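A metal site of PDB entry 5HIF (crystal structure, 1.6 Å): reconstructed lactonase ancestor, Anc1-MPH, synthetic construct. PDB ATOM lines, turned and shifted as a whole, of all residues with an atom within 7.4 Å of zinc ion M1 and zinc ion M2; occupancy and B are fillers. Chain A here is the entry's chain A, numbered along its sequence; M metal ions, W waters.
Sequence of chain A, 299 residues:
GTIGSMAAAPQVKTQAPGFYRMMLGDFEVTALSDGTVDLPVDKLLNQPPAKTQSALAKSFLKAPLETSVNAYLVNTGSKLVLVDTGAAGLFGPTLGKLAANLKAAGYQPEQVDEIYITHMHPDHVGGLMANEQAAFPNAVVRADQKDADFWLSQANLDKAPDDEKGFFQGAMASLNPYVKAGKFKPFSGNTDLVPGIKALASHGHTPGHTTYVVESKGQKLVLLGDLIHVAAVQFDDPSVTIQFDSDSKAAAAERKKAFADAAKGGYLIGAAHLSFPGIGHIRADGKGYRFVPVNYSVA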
ATOM      1  N   SER A  68      -0.613 -11.512  31.499  1.00  0.00           N
ATOM      2  CA  SER A  68       0.614 -11.244  32.235  1.00  0.00           C
ATOM      3  C   SER A  68       1.062  -9.790  32.090  1.00  0.00           C
ATOM      4  O   SER A  68       0.828  -9.162  31.094  1.00  0.00           O
ATOM      5  CB  SER A  68       1.682 -12.116  31.765  1.00  0.00           C
ATOM      6  OG  SER A  68       1.470 -13.474  32.201  1.00  0.00           O
ATOM      7  N   VAL A  69       1.734  -9.356  33.138  1.00  0.00           N
ATOM      8  CA  VAL A  69       2.424  -8.084  33.208  1.00  0.00           C
ATOM      9  C   VAL A  69       3.831  -8.350  33.632  1.00  0.00           C
ATOM     10  O   VAL A  69       4.077  -8.682  34.796  1.00  0.00           O
ATOM     11  CB  VAL A  69       1.767  -7.075  34.121  1.00  0.00           C
ATOM     12  CG1 VAL A  69       2.570  -5.704  34.158  1.00  0.00           C
ATOM     13  CG2 VAL A  69       0.319  -6.765  33.720  1.00  0.00           C
ATOM     14  N   ASN A  70       4.761  -8.174  32.721  1.00  0.00           N
ATOM     15  CA  ASN A  70       6.202  -8.578  32.927  1.00  0.00           C
ATOM     16  C   ASN A  70       7.122  -7.399  32.911  1.00  0.00           C
ATOM     17  O   ASN A  70       6.882  -6.404  32.197  1.00  0.00           O
ATOM     18  CB  ASN A  70       6.625  -9.545  31.872  1.00  0.00           C
ATOM     19  CG  ASN A  70       5.664 -10.722  31.608  1.00  0.00           C
ATOM     20  OD1 ASN A  70       5.048 -11.250  32.563  1.00  0.00           O
ATOM     21  ND2 ASN A  70       5.538 -11.149  30.356  1.00  0.00           N
ATOM     22  N   ASP A  84      11.136  -1.848  32.803  1.00  0.00           N
ATOM     23  CA  ASP A  84       9.790  -1.745  33.351  1.00  0.00           C
ATOM     24  C   ASP A  84       9.666  -2.207  34.813  1.00  0.00           C
ATOM     25  O   ASP A  84      10.598  -2.767  35.378  1.00  0.00           O
ATOM     26  CB  ASP A  84       8.782  -2.382  32.470  1.00  0.00           C
ATOM     27  CG  ASP A  84       8.617  -1.655  31.129  1.00  0.00           C
ATOM     28  OD1 ASP A  84       9.004  -0.465  31.062  1.00  0.00           O
ATOM     29  OD2 ASP A  84       8.042  -2.250  30.185  1.00  0.00           O
ATOM     30  N   THR A 118       9.668   1.229  28.944  1.00  0.00           N
ATOM     31  CA  THR A 118       9.266   1.111  27.561  1.00  0.00           C
ATOM     32  C   THR A 118       8.232   2.233  27.165  1.00  0.00           C
ATOM     33  O   THR A 118       8.350   2.827  26.126  1.00  0.00           O
ATOM     34  CB  THR A 118       8.671  -0.301  27.230  1.00  0.00           C
ATOM     35  OG1 THR A 118       7.523  -0.519  28.079  1.00  0.00           O
ATOM     36  CG2 THR A 118       9.731  -1.375  27.385  1.00  0.00           C
ATOM     37  N   HIS A 119       7.362   2.495  28.116  1.00  0.00           N
ATOM     38  CA  HIS A 119       6.373   3.569  27.971  1.00  0.00           C
ATOM     39  C   HIS A 119       5.684   3.814  29.270  1.00  0.00           C
ATOM     40  O   HIS A 119       5.684   2.961  30.160  1.00  0.00           O
ATOM     41  CB  HIS A 119       5.353   3.190  26.888  1.00  0.00           C
ATOM     42  CG  HIS A 119       4.477   2.012  27.215  1.00  0.00           C
ATOM     43  ND1 HIS A 119       4.978   0.730  27.451  1.00  0.00           N
ATOM     44  CD2 HIS A 119       3.129   1.914  27.273  1.00  0.00           C
ATOM     45  CE1 HIS A 119       3.974  -0.092  27.667  1.00  0.00           C
ATOM     46  NE2 HIS A 119       2.830   0.572  27.524  1.00  0.00           N
ATOM     47  N   MET A 120       5.097   4.992  29.419  1.00  0.00           N
ATOM     48  CA  MET A 120       4.573   5.383  30.731  1.00  0.00           C
ATOM     49  C   MET A 120       3.120   5.012  31.053  1.00  0.00           C
ATOM     50  O   MET A 120       2.459   5.720  31.801  1.00  0.00           O
ATOM     51  CB  MET A 120       4.808   6.898  30.968  1.00  0.00           C
ATOM     52  CG  MET A 120       6.307   7.193  30.948  1.00  0.00           C
ATOM     53  SD  MET A 120       6.600   8.956  31.342  1.00  0.00           S
ATOM     54  CE  MET A 120       8.369   8.973  31.129  1.00  0.00           C
ATOM     55  N   HIS A 121       2.661   3.886  30.575  1.00  0.00           N
ATOM     56  CA  HIS A 121       1.446   3.340  31.068  1.00  0.00           C
ATOM     57  C   HIS A 121       1.592   2.851  32.484  1.00  0.00           C
ATOM     58  O   HIS A 121       2.690   2.543  32.969  1.00  0.00           O
ATOM     59  CB  HIS A 121       0.969   2.226  30.121  1.00  0.00           C
ATOM     60  CG  HIS A 121       0.310   2.712  28.861  1.00  0.00           C
ATOM     61  ND1 HIS A 121       0.018   1.925  27.773  1.00  0.00           N
ATOM     62  CD2 HIS A 121      -0.120   3.974  28.524  1.00  0.00           C
ATOM     63  CE1 HIS A 121      -0.570   2.639  26.815  1.00  0.00           C
ATOM     64  NE2 HIS A 121      -0.660   3.867  27.276  1.00  0.00           N
ATOM     65  N   PRO A 122       0.477   2.801  33.226  1.00  0.00           N
ATOM     66  CA  PRO A 122       0.547   2.560  34.684  1.00  0.00           C
ATOM     67  C   PRO A 122       1.173   1.242  35.066  1.00  0.00           C
ATOM     68  O   PRO A 122       1.808   1.189  36.092  1.00  0.00           O
ATOM     69  CB  PRO A 122      -0.908   2.573  35.126  1.00  0.00           C
ATOM     70  CG  PRO A 122      -1.651   2.382  33.913  1.00  0.00           C
ATOM     71  CD  PRO A 122      -0.910   3.077  32.801  1.00  0.00           C
ATOM     72  N   ASP A 123       0.961   0.261  34.247  1.00  0.00           N
ATOM     73  CA  ASP A 123       1.479  -1.079  34.429  1.00  0.00           C
ATOM     74  C   ASP A 123       2.924  -1.220  34.065  1.00  0.00           C
ATOM     75  O   ASP A 123       3.464  -2.333  34.217  1.00  0.00           O
ATOM     76  CB  ASP A 123       0.618  -2.114  33.707  1.00  0.00           C
ATOM     77  CG  ASP A 123       0.471  -1.856  32.180  1.00  0.00           C
ATOM     78  OD1 ASP A 123       0.202  -0.700  31.824  1.00  0.00           O
ATOM     79  OD2 ASP A 123       0.677  -2.804  31.402  1.00  0.00           O
ATOM     80  N   HIS A 124       3.582  -0.137  33.723  1.00  0.00           N
ATOM     81  CA  HIS A 124       5.043  -0.099  33.509  1.00  0.00           C
ATOM     82  C   HIS A 124       5.794   0.786  34.416  1.00  0.00           C
ATOM     83  O   HIS A 124       6.981   0.510  34.737  1.00  0.00           O
ATOM     84  CB  HIS A 124       5.354   0.193  32.051  1.00  0.00           C
ATOM     85  CG  HIS A 124       4.660  -0.789  31.117  1.00  0.00           C
ATOM     86  ND1 HIS A 124       5.273  -1.866  30.533  1.00  0.00           N
ATOM     87  CD2 HIS A 124       3.342  -0.901  30.805  1.00  0.00           C
ATOM     88  CE1 HIS A 124       4.392  -2.579  29.862  1.00  0.00           C
ATOM     89  NE2 HIS A 124       3.183  -2.030  30.058  1.00  0.00           N
ATOM     90  N   PHE A 167      -4.191   7.670  33.733  1.00  0.00           N
ATOM     91  CA  PHE A 167      -2.925   7.285  33.171  1.00  0.00           C
ATOM     92  C   PHE A 167      -1.915   8.420  33.392  1.00  0.00           C
ATOM     93  O   PHE A 167      -0.717   8.159  33.710  1.00  0.00           O
ATOM     94  CB  PHE A 167      -2.962   6.961  31.671  1.00  0.00           C
ATOM     95  CG  PHE A 167      -3.712   5.708  31.334  1.00  0.00           C
ATOM     96  CD1 PHE A 167      -4.456   4.987  32.295  1.00  0.00           C
ATOM     97  CD2 PHE A 167      -3.706   5.271  30.000  1.00  0.00           C
ATOM     98  CE1 PHE A 167      -5.152   3.838  31.925  1.00  0.00           C
ATOM     99  CE2 PHE A 167      -4.394   4.117  29.633  1.00  0.00           C
ATOM    100  CZ  PHE A 167      -5.126   3.412  30.591  1.00  0.00           C
ATOM    101  N   HIS A 205       2.313   2.708  20.072  1.00  0.00           N
ATOM    102  CA  HIS A 205       1.530   2.374  21.230  1.00  0.00           C
ATOM    103  C   HIS A 205       1.384   3.551  22.202  1.00  0.00           C
ATOM    104  O   HIS A 205       0.350   3.812  22.792  1.00  0.00           O
ATOM    105  CB  HIS A 205       2.148   1.160  21.948  1.00  0.00           C
ATOM    106  CG  HIS A 205       1.406   0.736  23.181  1.00  0.00           C
ATOM    107  ND1 HIS A 205       0.087   0.246  23.169  1.00  0.00           N
ATOM    108  CD2 HIS A 205       1.786   0.754  24.474  1.00  0.00           C
ATOM    109  CE1 HIS A 205      -0.286   0.034  24.416  1.00  0.00           C
ATOM    110  NE2 HIS A 205       0.744   0.279  25.214  1.00  0.00           N
ATOM    111  N   THR A 206       2.484   4.245  22.407  1.00  0.00           N
ATOM    112  CA  THR A 206       2.547   5.599  22.991  1.00  0.00           C
ATOM    113  C   THR A 206       3.520   6.433  22.116  1.00  0.00           C
ATOM    114  O   THR A 206       4.330   5.901  21.413  1.00  0.00           O
ATOM    115  CB  THR A 206       2.953   5.554  24.453  1.00  0.00           C
ATOM    116  OG1 THR A 206       4.361   5.224  24.528  1.00  0.00           O
ATOM    117  CG2 THR A 206       2.060   4.657  25.296  1.00  0.00           C
ATOM    118  N   HIS A 209       7.042   5.150  22.836  1.00  0.00           N
ATOM    119  CA  HIS A 209       7.234   3.755  23.144  1.00  0.00           C
ATOM    120  C   HIS A 209       8.607   3.300  22.608  1.00  0.00           C
ATOM    121  O   HIS A 209       8.948   3.590  21.459  1.00  0.00           O
ATOM    122  CB  HIS A 209       6.081   2.917  22.562  1.00  0.00           C
ATOM    123  CG  HIS A 209       6.179   1.471  22.976  1.00  0.00           C
ATOM    124  ND1 HIS A 209       7.036   0.599  22.358  1.00  0.00           N
ATOM    125  CD2 HIS A 209       5.578   0.789  23.958  1.00  0.00           C
ATOM    126  CE1 HIS A 209       6.966  -0.577  22.984  1.00  0.00           C
ATOM    127  NE2 HIS A 209       6.062  -0.506  23.922  1.00  0.00           N
ATOM    128  N   GLY A 225       8.342  -4.337  25.071  1.00  0.00           N
ATOM    129  CA  GLY A 225       7.287  -3.548  25.747  1.00  0.00           C
ATOM    130  C   GLY A 225       5.899  -4.044  25.378  1.00  0.00           C
ATOM    131  O   GLY A 225       5.616  -5.224  25.490  1.00  0.00           O
ATOM    132  N   ASP A 226       5.114  -3.102  24.893  1.00  0.00           N
ATOM    133  CA  ASP A 226       3.729  -3.381  24.493  1.00  0.00           C
ATOM    134  C   ASP A 226       3.499  -3.370  22.994  1.00  0.00           C
ATOM    135  O   ASP A 226       2.426  -2.942  22.519  1.00  0.00           O
ATOM    136  CB  ASP A 226       2.766  -2.380  25.195  1.00  0.00           C
ATOM    137  CG  ASP A 226       2.528  -2.712  26.655  1.00  0.00           C
ATOM    138  OD1 ASP A 226       3.290  -3.535  27.218  1.00  0.00           O
ATOM    139  OD2 ASP A 226       1.600  -2.088  27.261  1.00  0.00           O
ATOM    140  N   ILE A 228       2.770  -6.009  21.621  1.00  0.00           N
ATOM    141  CA  ILE A 228       1.719  -7.065  21.529  1.00  0.00           C
ATOM    142  C   ILE A 228       0.959  -7.114  22.839  1.00  0.00           C
ATOM    143  O   ILE A 228       1.513  -6.854  23.898  1.00  0.00           O
ATOM    144  CB  ILE A 228       2.332  -8.379  21.076  1.00  0.00           C
ATOM    145  CG1 ILE A 228       1.271  -9.447  20.881  1.00  0.00           C
ATOM    146  CG2 ILE A 228       3.339  -8.805  22.045  1.00  0.00           C
ATOM    147  CD1 ILE A 228       1.628 -10.568  19.945  1.00  0.00           C
ATOM    148  N   HIS A 229      -0.357  -7.354  22.786  1.00  0.00           N
ATOM    149  CA  HIS A 229      -1.181  -7.577  23.916  1.00  0.00           C
ATOM    150  C   HIS A 229      -1.852  -8.945  24.003  1.00  0.00           C
ATOM    151  O   HIS A 229      -2.113  -9.398  25.116  1.00  0.00           O
ATOM    152  CB  HIS A 229      -2.282  -6.524  24.098  1.00  0.00           C
ATOM    153  CG  HIS A 229      -1.750  -5.155  24.421  1.00  0.00           C
ATOM    154  ND1 HIS A 229      -1.117  -4.362  23.486  1.00  0.00           N
ATOM    155  CD2 HIS A 229      -1.733  -4.469  25.582  1.00  0.00           C
ATOM    156  CE1 HIS A 229      -0.753  -3.238  24.056  1.00  0.00           C
ATOM    157  NE2 HIS A 229      -1.143  -3.263  25.309  1.00  0.00           N
ATOM    158  N   PHE A 244      -5.794   0.551  23.663  1.00  0.00           N
ATOM    159  CA  PHE A 244      -4.739   1.128  24.474  1.00  0.00           C
ATOM    160  C   PHE A 244      -3.652   1.862  23.624  1.00  0.00           C
ATOM    161  O   PHE A 244      -2.842   2.578  24.178  1.00  0.00           O
ATOM    162  CB  PHE A 244      -4.038   0.035  25.286  1.00  0.00           C
ATOM    163  CG  PHE A 244      -4.908  -0.709  26.245  1.00  0.00           C
ATOM    164  CD1 PHE A 244      -5.874  -0.069  26.998  1.00  0.00           C
ATOM    165  CD2 PHE A 244      -4.741  -2.090  26.398  1.00  0.00           C
ATOM    166  CE1 PHE A 244      -6.655  -0.761  27.903  1.00  0.00           C
ATOM    167  CE2 PHE A 244      -5.524  -2.770  27.299  1.00  0.00           C
ATOM    168  CZ  PHE A 244      -6.446  -2.080  28.086  1.00  0.00           C
ATOM    169  N   ASP A 245      -3.553   1.627  22.329  1.00  0.00           N
ATOM    170  CA  ASP A 245      -2.615   2.306  21.482  1.00  0.00           C
ATOM    171  C   ASP A 245      -2.935   3.768  21.315  1.00  0.00           C
ATOM    172  O   ASP A 245      -4.076   4.109  20.982  1.00  0.00           O
ATOM    173  CB  ASP A 245      -2.541   1.708  20.079  1.00  0.00           C
ATOM    174  CG  ASP A 245      -2.080   0.237  20.070  1.00  0.00           C
ATOM    175  OD1 ASP A 245      -1.137  -0.144  20.837  1.00  0.00           O
ATOM    176  OD2 ASP A 245      -2.565  -0.512  19.184  1.00  0.00           O
ATOM    177  N   ALA A 272       6.051  -7.579  27.523  1.00  0.00           N
ATOM    178  CA  ALA A 272       5.358  -7.300  28.790  1.00  0.00           C
ATOM    179  C   ALA A 272       4.053  -8.023  28.984  1.00  0.00           C
ATOM    180  O   ALA A 272       3.723  -8.343  30.153  1.00  0.00           O
ATOM    181  CB  ALA A 272       5.087  -5.780  28.918  1.00  0.00           C
ATOM    182  N   HIS A 273       3.381  -8.357  27.876  1.00  0.00           N
ATOM    183  CA  HIS A 273       2.030  -8.954  27.973  1.00  0.00           C
ATOM    184  C   HIS A 273       1.914 -10.315  27.278  1.00  0.00           C
ATOM    185  O   HIS A 273       0.792 -10.777  27.035  1.00  0.00           O
ATOM    186  CB  HIS A 273       0.895  -7.954  27.534  1.00  0.00           C
ATOM    187  CG  HIS A 273       0.919  -6.691  28.349  1.00  0.00           C
ATOM    188  ND1 HIS A 273       0.916  -6.674  29.711  1.00  0.00           N
ATOM    189  CD2 HIS A 273       0.971  -5.423  27.957  1.00  0.00           C
ATOM    190  CE1 HIS A 273       0.953  -5.415  30.151  1.00  0.00           C
ATOM    191  NE2 HIS A 273       1.021  -4.651  29.108  1.00  0.00           N
HETATM  192 ZN    ZN M   1       0.752  -0.093  27.406  1.00  0.00          ZN
HETATM  193 ZN    ZN M   2       1.315  -2.616  29.360  1.00  0.00          ZN
HETATM  194  O   HOH W   1       0.337  -0.910  29.118  1.00  0.00           O
HETATM  195  O   HOH W   2      -1.330  -0.951  26.966  1.00  0.00           O
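A ring nitrogen (ND1) of His 273 sits at hydrogen-bond distance from the backbone carbonyl oxygen (O) of Ser 68, 2.8 Å away. A ring nitrogen (ND1) of His 124 lies within hydrogen-bond range of the side-chain carboxylate (OD2) of Asp 84, 2.8 Å away. The backbone NH of Asp 226 lies within hydrogen-bond range of a ring nitrogen (NE2) of His 209 (2.9 Å). The side-chain hydroxyl (OG1) of Thr 118 sits at hydrogen-bond distance from a ring nitrogen (ND1) of His 119 (2.9 Å). A ring nitrogen (ND1) of His 205 sits at hydrogen-bond distance from the side-chain carboxylate (OD1) of Asp 245 (2.7 Å).
Within 4 Å of zinc ion M1: His 119, His 121, His 205 and Asp 226.
Five residues have an atom within 4 Å of zinc ion M2: His 119, Asp 123, His 124, Asp 226 and His 273. Along chain A the residues within 4 Å of zinc ion M2 span positions 119 to 273. The nearest printed residue that does not touch zinc ion M2 is His 229 (4.8 Å).
Zinc ion M1 is bound by water W1 (1.9 Å), the side-chain carboxylate (OD2) of Asp 226 (2.2 Å), a ring nitrogen (ND1) of His 121 (2.2 Å), a ring nitrogen (NE2) of His 119 (2.2 Å), a ring nitrogen (NE2) of His 205 (2.2 Å) and water W2 (2.3 Å). Zinc ion M1 has six donor atoms within binding distance.
Zinc ion M2 is bound by water W1 (2.0 Å), NE2 of His 273 (2.1 Å), NE2 of His 124 (2.1 Å), OD2 of Asp 123 (2.1 Å) and OD2 of Asp 226 (2.2 Å).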
